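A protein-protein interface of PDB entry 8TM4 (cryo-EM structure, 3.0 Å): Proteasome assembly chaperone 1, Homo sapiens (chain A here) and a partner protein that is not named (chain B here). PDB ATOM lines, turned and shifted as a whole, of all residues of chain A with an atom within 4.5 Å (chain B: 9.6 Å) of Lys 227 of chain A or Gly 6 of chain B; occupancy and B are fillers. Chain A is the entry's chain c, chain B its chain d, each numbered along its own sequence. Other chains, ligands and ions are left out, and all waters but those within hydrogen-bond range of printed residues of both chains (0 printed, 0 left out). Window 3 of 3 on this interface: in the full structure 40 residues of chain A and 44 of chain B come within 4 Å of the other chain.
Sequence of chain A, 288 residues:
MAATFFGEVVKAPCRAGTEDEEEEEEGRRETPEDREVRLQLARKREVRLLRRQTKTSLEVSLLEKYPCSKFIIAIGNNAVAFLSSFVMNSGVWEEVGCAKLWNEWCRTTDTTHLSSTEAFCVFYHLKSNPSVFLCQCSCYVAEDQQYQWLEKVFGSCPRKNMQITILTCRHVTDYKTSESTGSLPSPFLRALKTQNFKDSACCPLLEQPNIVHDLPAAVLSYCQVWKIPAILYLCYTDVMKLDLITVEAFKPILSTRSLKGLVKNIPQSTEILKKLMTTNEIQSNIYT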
ATOM      1  N   LYS A 160      18.898   2.554  -2.361  1.00  0.00           N
ATOM      2  CA  LYS A 160      17.512   3.059  -2.160  1.00  0.00           C
ATOM      3  C   LYS A 160      17.248   4.211  -3.135  1.00  0.00           C
ATOM      4  O   LYS A 160      16.336   5.015  -2.862  1.00  0.00           O
ATOM      5  CB  LYS A 160      17.289   3.501  -0.711  1.00  0.00           C
ATOM      6  N   GLN A 195       7.526  -1.054   0.513  1.00  0.00           N
ATOM      7  CA  GLN A 195       7.282   0.139   1.369  1.00  0.00           C
ATOM      8  C   GLN A 195       7.653   1.412   0.594  1.00  0.00           C
ATOM      9  O   GLN A 195       6.749   2.240   0.362  1.00  0.00           O
ATOM     10  CB  GLN A 195       8.067   0.003   2.678  1.00  0.00           C
ATOM     11  CG  GLN A 195       7.964   1.208   3.604  1.00  0.00           C
ATOM     12  CD  GLN A 195       9.223   2.044   3.609  1.00  0.00           C
ATOM     13  OE1 GLN A 195      10.290   1.590   4.019  1.00  0.00           O
ATOM     14  NE2 GLN A 195       9.108   3.284   3.162  1.00  0.00           N
ATOM     15  N   ASN A 196       8.930   1.565   0.223  1.00  0.00           N
ATOM     16  CA  ASN A 196       9.461   2.744  -0.517  1.00  0.00           C
ATOM     17  C   ASN A 196       8.644   2.974  -1.791  1.00  0.00           C
ATOM     18  O   ASN A 196       8.088   4.078  -1.931  1.00  0.00           O
ATOM     19  CB  ASN A 196      10.946   2.610  -0.869  1.00  0.00           C
ATOM     20  CG  ASN A 196      11.854   3.245   0.164  1.00  0.00           C
ATOM     21  OD1 ASN A 196      11.520   3.291   1.345  1.00  0.00           O
ATOM     22  ND2 ASN A 196      13.002   3.744  -0.266  1.00  0.00           N
ATOM     23  N   CYS A 223      15.210  -5.688  -1.334  1.00  0.00           N
ATOM     24  CA  CYS A 223      14.839  -4.266  -1.563  1.00  0.00           C
ATOM     25  C   CYS A 223      14.115  -3.730  -0.326  1.00  0.00           C
ATOM     26  O   CYS A 223      14.456  -2.628   0.117  1.00  0.00           O
ATOM     27  CB  CYS A 223      13.987  -4.110  -2.817  1.00  0.00           C
ATOM     28  SG  CYS A 223      14.932  -4.374  -4.340  1.00  0.00           S
ATOM     29  N   GLN A 224      13.183  -4.510   0.225  1.00  0.00           N
ATOM     30  CA  GLN A 224      12.299  -4.099   1.350  1.00  0.00           C
ATOM     31  C   GLN A 224      13.142  -3.887   2.612  1.00  0.00           C
ATOM     32  O   GLN A 224      12.901  -2.879   3.307  1.00  0.00           O
ATOM     33  CB  GLN A 224      11.172  -5.122   1.532  1.00  0.00           C
ATOM     34  CG  GLN A 224      10.372  -5.010   2.829  1.00  0.00           C
ATOM     35  CD  GLN A 224       9.528  -3.762   2.944  1.00  0.00           C
ATOM     36  OE1 GLN A 224      10.007  -2.642   2.784  1.00  0.00           O
ATOM     37  NE2 GLN A 224       8.259  -3.942   3.272  1.00  0.00           N
ATOM     38  N   VAL A 225      14.098  -4.775   2.894  1.00  0.00           N
ATOM     39  CA  VAL A 225      14.878  -4.730   4.167  1.00  0.00           C
ATOM     40  C   VAL A 225      15.817  -3.515   4.131  1.00  0.00           C
ATOM     41  O   VAL A 225      16.054  -2.930   5.207  1.00  0.00           O
ATOM     42  CB  VAL A 225      15.630  -6.041   4.481  1.00  0.00           C
ATOM     43  CG1 VAL A 225      16.671  -6.426   3.439  1.00  0.00           C
ATOM     44  CG2 VAL A 225      16.263  -5.978   5.860  1.00  0.00           C
ATOM     45  N   TRP A 226      16.282  -3.123   2.940  1.00  0.00           N
ATOM     46  CA  TRP A 226      17.140  -1.925   2.727  1.00  0.00           C
ATOM     47  C   TRP A 226      16.302  -0.779   2.148  1.00  0.00           C
ATOM     48  O   TRP A 226      16.899   0.135   1.549  1.00  0.00           O
ATOM     49  CB  TRP A 226      18.334  -2.261   1.830  1.00  0.00           C
ATOM     50  CG  TRP A 226      19.053  -3.522   2.199  1.00  0.00           C
ATOM     51  CD1 TRP A 226      19.229  -4.616   1.407  1.00  0.00           C
ATOM     52  CD2 TRP A 226      19.705  -3.822   3.446  1.00  0.00           C
ATOM     53  NE1 TRP A 226      19.937  -5.579   2.071  1.00  0.00           N
ATOM     54  CE2 TRP A 226      20.245  -5.121   3.323  1.00  0.00           C
ATOM     55  CE3 TRP A 226      19.887  -3.129   4.648  1.00  0.00           C
ATOM     56  CZ2 TRP A 226      20.949  -5.734   4.357  1.00  0.00           C
ATOM     57  CZ3 TRP A 226      20.585  -3.737   5.668  1.00  0.00           C
ATOM     58  CH2 TRP A 226      21.108  -5.022   5.523  1.00  0.00           C
ATOM     59  N   LYS A 227      14.982  -0.822   2.367  1.00  0.00           N
ATOM     60  CA  LYS A 227      13.972   0.169   1.903  1.00  0.00           C
ATOM     61  C   LYS A 227      14.425   0.793   0.575  1.00  0.00           C
ATOM     62  O   LYS A 227      14.984   1.907   0.592  1.00  0.00           O
ATOM     63  CB  LYS A 227      13.687   1.186   3.017  1.00  0.00           C
ATOM     64  CG  LYS A 227      14.890   1.674   3.818  1.00  0.00           C
ATOM     65  CD  LYS A 227      14.547   2.683   4.901  1.00  0.00           C
ATOM     66  CE  LYS A 227      13.730   2.131   6.054  1.00  0.00           C
ATOM     67  NZ  LYS A 227      14.380   0.972   6.712  1.00  0.00           N
ATOM     68  N   ILE A 228      14.168   0.078  -0.527  1.00  0.00           N
ATOM     69  CA  ILE A 228      14.498   0.456  -1.933  1.00  0.00           C
ATOM     70  C   ILE A 228      13.185   0.444  -2.724  1.00  0.00           C
ATOM     71  O   ILE A 228      12.377  -0.464  -2.468  1.00  0.00           O
ATOM     72  CB  ILE A 228      15.537  -0.523  -2.529  1.00  0.00           C
ATOM     73  CG1 ILE A 228      16.765  -0.667  -1.622  1.00  0.00           C
ATOM     74  CG2 ILE A 228      15.908  -0.141  -3.957  1.00  0.00           C
ATOM     75  CD1 ILE A 228      17.917  -1.447  -2.217  1.00  0.00           C
ATOM     76  N   PHE B   2      19.436  -8.735  12.484  1.00  0.00           N
ATOM     77  CA  PHE B   2      18.197  -7.915  12.529  1.00  0.00           C
ATOM     78  C   PHE B   2      18.459  -6.552  11.880  1.00  0.00           C
ATOM     79  O   PHE B   2      19.481  -5.914  12.203  1.00  0.00           O
ATOM     80  CB  PHE B   2      17.678  -7.741  13.958  1.00  0.00           C
ATOM     81  CG  PHE B   2      16.578  -6.717  14.083  1.00  0.00           C
ATOM     82  CD1 PHE B   2      15.381  -6.881  13.403  1.00  0.00           C
ATOM     83  CD2 PHE B   2      16.739  -5.581  14.862  1.00  0.00           C
ATOM     84  CE1 PHE B   2      14.373  -5.936  13.502  1.00  0.00           C
ATOM     85  CE2 PHE B   2      15.725  -4.640  14.962  1.00  0.00           C
ATOM     86  CZ  PHE B   2      14.547  -4.820  14.282  1.00  0.00           C
ATOM     87  N   VAL B   3      17.550  -6.137  10.991  1.00  0.00           N
ATOM     88  CA  VAL B   3      17.527  -4.813  10.302  1.00  0.00           C
ATOM     89  C   VAL B   3      16.153  -4.185  10.569  1.00  0.00           C
ATOM     90  O   VAL B   3      15.151  -4.858  10.271  1.00  0.00           O
ATOM     91  CB  VAL B   3      17.776  -4.974   8.790  1.00  0.00           C
ATOM     92  CG1 VAL B   3      17.791  -3.635   8.065  1.00  0.00           C
ATOM     93  CG2 VAL B   3      19.046  -5.761   8.498  1.00  0.00           C
ATOM     94  N   PRO B   4      16.035  -2.947  11.104  1.00  0.00           N
ATOM     95  CA  PRO B   4      14.719  -2.367  11.387  1.00  0.00           C
ATOM     96  C   PRO B   4      13.988  -1.928  10.107  1.00  0.00           C
ATOM     97  O   PRO B   4      14.646  -1.694   9.109  1.00  0.00           O
ATOM     98  CB  PRO B   4      15.037  -1.162  12.280  1.00  0.00           C
ATOM     99  CG  PRO B   4      16.429  -0.747  11.861  1.00  0.00           C
ATOM    100  CD  PRO B   4      17.124  -2.034  11.468  1.00  0.00           C
ATOM    101  N   CYS B   5      12.656  -1.821  10.180  1.00  0.00           N
ATOM    102  CA  CYS B   5      11.767  -1.307   9.101  1.00  0.00           C
ATOM    103  C   CYS B   5      11.699   0.224   9.161  1.00  0.00           C
ATOM    104  O   CYS B   5      11.201   0.826   8.187  1.00  0.00           O
ATOM    105  CB  CYS B   5      10.371  -1.911   9.207  1.00  0.00           C
ATOM    106  SG  CYS B   5       9.608  -1.681  10.834  1.00  0.00           S
ATOM    107  N   GLY B   6      12.185   0.816  10.259  1.00  0.00           N
ATOM    108  CA  GLY B   6      12.461   2.258  10.401  1.00  0.00           C
ATOM    109  C   GLY B   6      13.953   2.526  10.484  1.00  0.00           C
ATOM    110  O   GLY B   6      14.731   1.645  10.072  1.00  0.00           O
ATOM    111  N   GLU B   7      14.337   3.698  10.995  1.00  0.00           N
ATOM    112  CA  GLU B   7      15.748   4.167  11.045  1.00  0.00           C
ATOM    113  C   GLU B   7      16.535   3.286  12.022  1.00  0.00           C
ATOM    114  O   GLU B   7      17.516   2.654  11.583  1.00  0.00           O
ATOM    115  CB  GLU B   7      15.809   5.648  11.435  1.00  0.00           C
ATOM    116  CG  GLU B   7      17.220   6.194  11.595  1.00  0.00           C
ATOM    117  CD  GLU B   7      18.142   5.995  10.404  1.00  0.00           C
ATOM    118  OE1 GLU B   7      19.320   5.650  10.625  1.00  0.00           O
ATOM    119  OE2 GLU B   7      17.686   6.197   9.261  1.00  0.00           O
ATOM    120  N   SER B   8      16.107   3.249  13.288  1.00  0.00           N
ATOM    121  CA  SER B   8      16.857   2.680  14.438  1.00  0.00           C
ATOM    122  C   SER B   8      16.255   1.330  14.838  1.00  0.00           C
ATOM    123  O   SER B   8      15.047   1.131  14.604  1.00  0.00           O
ATOM    124  CB  SER B   8      16.869   3.641  15.597  1.00  0.00           C
ATOM    125  N   ALA B   9      17.077   0.454  15.427  1.00  0.00           N
ATOM    126  CA  ALA B   9      16.698  -0.890  15.921  1.00  0.00           C
ATOM    127  C   ALA B   9      16.133  -0.756  17.341  1.00  0.00           C
ATOM    128  O   ALA B   9      16.899  -0.326  18.225  1.00  0.00           O
ATOM    129  CB  ALA B   9      17.890  -1.815  15.883  1.00  0.00           C
ATOM    130  N   PRO B  10      14.846  -1.080  17.620  1.00  0.00           N
ATOM    131  CA  PRO B  10      14.313  -1.001  18.986  1.00  0.00           C
ATOM    132  C   PRO B  10      15.154  -1.794  19.997  1.00  0.00           C
ATOM    133  O   PRO B  10      15.721  -2.805  19.618  1.00  0.00           O
ATOM    134  CB  PRO B  10      12.912  -1.615  18.866  1.00  0.00           C
ATOM    135  CG  PRO B  10      12.523  -1.301  17.447  1.00  0.00           C
ATOM    136  CD  PRO B  10      13.807  -1.510  16.671  1.00  0.00           C
ATOM    137  N   LYS B  43       5.552  -4.771  13.914  1.00  0.00           N
ATOM    138  CA  LYS B  43       6.829  -5.062  13.210  1.00  0.00           C
ATOM    139  C   LYS B  43       7.909  -4.096  13.710  1.00  0.00           C
ATOM    140  O   LYS B  43       7.735  -2.875  13.533  1.00  0.00           O
ATOM    141  CB  LYS B  43       6.639  -4.967  11.692  1.00  0.00           C
ATOM    142  CG  LYS B  43       7.809  -5.470  10.857  1.00  0.00           C
ATOM    143  CD  LYS B  43       7.687  -5.188   9.370  1.00  0.00           C
ATOM    144  CE  LYS B  43       6.498  -5.864   8.716  1.00  0.00           C
ATOM    145  NZ  LYS B  43       6.557  -5.776   7.237  1.00  0.00           N
ATOM    146  N   ILE B  44       8.979  -4.632  14.310  1.00  0.00           N
ATOM    147  CA  ILE B  44      10.242  -3.889  14.609  1.00  0.00           C
ATOM    148  C   ILE B  44      11.100  -3.879  13.340  1.00  0.00           C
ATOM    149  O   ILE B  44      11.844  -2.900  13.143  1.00  0.00           O
ATOM    150  CB  ILE B  44      10.993  -4.462  15.835  1.00  0.00           C
ATOM    151  CG1 ILE B  44      11.440  -5.921  15.670  1.00  0.00           C
ATOM    152  CG2 ILE B  44      10.154  -4.279  17.088  1.00  0.00           C
ATOM    153  CD1 ILE B  44      12.488  -6.363  16.671  1.00  0.00           C
ATOM    154  N   GLY B  45      10.963  -4.916  12.506  1.00  0.00           N
ATOM    155  CA  GLY B  45      11.554  -5.000  11.160  1.00  0.00           C
ATOM    156  C   GLY B  45      11.695  -6.441  10.708  1.00  0.00           C
ATOM    157  O   GLY B  45      10.710  -7.193  10.829  1.00  0.00           O
ATOM    158  N   TYR B  46      12.877  -6.805  10.205  1.00  0.00           N
ATOM    159  CA  TYR B  46      13.165  -8.074   9.492  1.00  0.00           C
ATOM    160  C   TYR B  46      14.434  -8.679  10.090  1.00  0.00           C
ATOM    161  O   TYR B  46      15.427  -7.942  10.200  1.00  0.00           O
ATOM    162  CB  TYR B  46      13.342  -7.812   7.993  1.00  0.00           C
ATOM    163  CG  TYR B  46      12.506  -6.675   7.464  1.00  0.00           C
ATOM    164  CD1 TYR B  46      11.213  -6.887   7.020  1.00  0.00           C
ATOM    165  CD2 TYR B  46      12.997  -5.381   7.429  1.00  0.00           C
ATOM    166  CE1 TYR B  46      10.433  -5.847   6.542  1.00  0.00           C
ATOM    167  CE2 TYR B  46      12.231  -4.330   6.957  1.00  0.00           C
ATOM    168  CZ  TYR B  46      10.942  -4.563   6.510  1.00  0.00           C
ATOM    169  OH  TYR B  46      10.163  -3.544   6.038  1.00  0.00           O
ATOM    170  N   TYR B  48      16.508 -10.397   8.566  1.00  0.00           N
ATOM    171  CA  TYR B  48      16.837 -10.728   7.156  1.00  0.00           C
ATOM    172  C   TYR B  48      18.161 -11.495   7.130  1.00  0.00           C
ATOM    173  O   TYR B  48      19.156 -11.005   7.702  1.00  0.00           O
ATOM    174  CB  TYR B  48      16.887  -9.467   6.292  1.00  0.00           C
ATOM    175  CG  TYR B  48      17.342  -9.686   4.870  1.00  0.00           C
ATOM    176  CD1 TYR B  48      16.466 -10.150   3.903  1.00  0.00           C
ATOM    177  CD2 TYR B  48      18.644  -9.413   4.484  1.00  0.00           C
ATOM    178  CE1 TYR B  48      16.873 -10.349   2.594  1.00  0.00           C
ATOM    179  CE2 TYR B  48      19.066  -9.602   3.178  1.00  0.00           C
ATOM    180  CZ  TYR B  48      18.177 -10.071   2.227  1.00  0.00           C
ATOM    181  OH  TYR B  48      18.567 -10.271   0.933  1.00  0.00           O
ATOM    182  N   GLU B  70       1.178  -3.710   3.077  1.00  0.00           N
ATOM    183  CA  GLU B  70       2.500  -4.028   3.684  1.00  0.00           C
ATOM    184  C   GLU B  70       2.969  -5.396   3.176  1.00  0.00           C
ATOM    185  O   GLU B  70       2.106  -6.271   2.977  1.00  0.00           O
ATOM    186  CB  GLU B  70       2.427  -4.018   5.214  1.00  0.00           C
ATOM    187  CG  GLU B  70       2.131  -2.651   5.813  1.00  0.00           C
ATOM    188  CD  GLU B  70       3.171  -1.577   5.537  1.00  0.00           C
ATOM    189  OE1 GLU B  70       2.776  -0.403   5.396  1.00  0.00           O
ATOM    190  OE2 GLU B  70       4.371  -1.913   5.471  1.00  0.00           O
ATOM    191  N   LEU B  71       4.284  -5.563   2.995  1.00  0.00           N
ATOM    192  CA  LEU B  71       4.911  -6.698   2.264  1.00  0.00           C
ATOM    193  C   LEU B  71       5.442  -7.722   3.276  1.00  0.00           C
ATOM    194  O   LEU B  71       6.134  -7.309   4.229  1.00  0.00           O
ATOM    195  CB  LEU B  71       6.038  -6.160   1.374  1.00  0.00           C
ATOM    196  CG  LEU B  71       6.595  -7.136   0.335  1.00  0.00           C
ATOM    197  CD1 LEU B  71       5.731  -7.156  -0.918  1.00  0.00           C
ATOM    198  CD2 LEU B  71       8.035  -6.784  -0.020  1.00  0.00           C
ATOM    199  N   ILE B  73       7.962 -10.900   4.369  1.00  0.00           N
ATOM    200  CA  ILE B  73       9.409 -11.229   4.174  1.00  0.00           C
ATOM    201  C   ILE B  73       9.685 -12.581   4.846  1.00  0.00           C
ATOM    202  O   ILE B  73       9.068 -12.845   5.892  1.00  0.00           O
ATOM    203  CB  ILE B  73      10.310 -10.099   4.728  1.00  0.00           C
ATOM    204  CG1 ILE B  73      10.060  -8.751   4.039  1.00  0.00           C
ATOM    205  CG2 ILE B  73      11.783 -10.480   4.676  1.00  0.00           C
ATOM    206  CD1 ILE B  73      10.543  -8.676   2.609  1.00  0.00           C
ATOM    207  N   VAL B  77      10.156  -9.961  12.161  1.00  0.00           N
ATOM    208  CA  VAL B  77      10.172  -9.955  13.656  1.00  0.00           C
ATOM    209  C   VAL B  77       9.320  -8.777  14.151  1.00  0.00           C
ATOM    210  O   VAL B  77       9.298  -7.732  13.471  1.00  0.00           O
ATOM    211  CB  VAL B  77      11.613  -9.920  14.206  1.00  0.00           C
ATOM    212  CG1 VAL B  77      12.454  -8.822  13.570  1.00  0.00           C
ATOM    213  CG2 VAL B  77      11.658  -9.835  15.728  1.00  0.00           C
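The side-chain hydroxyl (OH) of Tyr 46 of chain B sits close to the side-chain amide oxygen (OE1) of Gln 224 of chain A, at 3.4 Å. NZ of Lys 227 of chain A is in hydrogen-bond range of O of Gly 6 of chain B (3.4 Å).
The side-chain amide nitrogen of Asn 196 of chain A sits at hydrogen-bond distance from the backbone carbonyl oxygen of Lys 227 of chain A, at 2.8 Å. The backbone carbonyl oxygen (O) of Tyr 46 of chain B sits at hydrogen-bond distance from the backbone NH (N) of Val 3 of chain B (2.9 Å). O of Lys 43 of chain B is in hydrogen-bond range of SG of Cys 5 of chain B, 3.5 Å away. The backbone NH (N) of Cys 5 of chain B is in hydrogen-bond range of the backbone carbonyl oxygen (O) of Ile 44 of chain B, 3.3 Å away. NZ of Lys 43 of chain B sits at hydrogen-bond distance from O of Leu 71 of chain B, 3.4 Å away.
Among the printed residues, merely in contact across the chains: Val 225 of chain A with Val 3 of chain B (3.4 Å), Lys 227 of chain A with Cys 5 of chain B (3.5 Å), Val 225 of chain A with Tyr 48 of chain B (3.6 Å), Lys 227 of chain A with Pro 4 of chain B (3.6 Å), Gln 224 of chain A with Leu 71 of chain B (3.7 Å), Val 225 of chain A with Tyr 46 of chain B (3.7 Å), Gln 224 of chain A with Ile 73 of chain B (3.7 Å) and Trp 226 of chain A with Val 3 of chain B (3.7 Å).
Lys 227 of chain A touches just these residues of chain B: Pro 4, Cys 5 and Gly 6. Gly 6 of chain B touches just one residue of chain A: Lys 227 (3.4 Å). Lys 160 of chain A touches none of the printed residues of chain B. Ile 228 of chain A touches none of the printed residues of chain B. Printed residues of chain A within 4 Å of Tyr 46 of chain B: Gln 224 (3.2 Å) and Val 225 (3.7 Å). Of the printed residues of chain A, Val 3 of chain B touches Val 225 and Trp 226. The nearest residue of chain B that does not touch Lys 227 of chain A is Glu 7 of chain B (5.1 Å). The nearest printed residue of chain A that does not touch Gly 6 of chain B is Gln 195 of chain A (6.6 Å).
Of the 9 printed residues of chain A, 4 touch a printed residue of chain B. Hydrophobic or aromatic side chains of chain A that line the printed part of chain B: Val 225 and Trp 226. Hydrophobic or aromatic side chains of chain B within 4 Å of the printed part of chain A: Val 3, Tyr 46, Tyr 48, Leu 71 and Ile 73. Along chain B the printed residues that touch a printed residue of chain A span positions 3 to 73. Among the printed residues, 10 pairs touch across the chains. Among the printed residues, no Asp or Glu carboxylate lies within 4 Å of a Lys or Arg side-chain nitrogen of the other chain.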
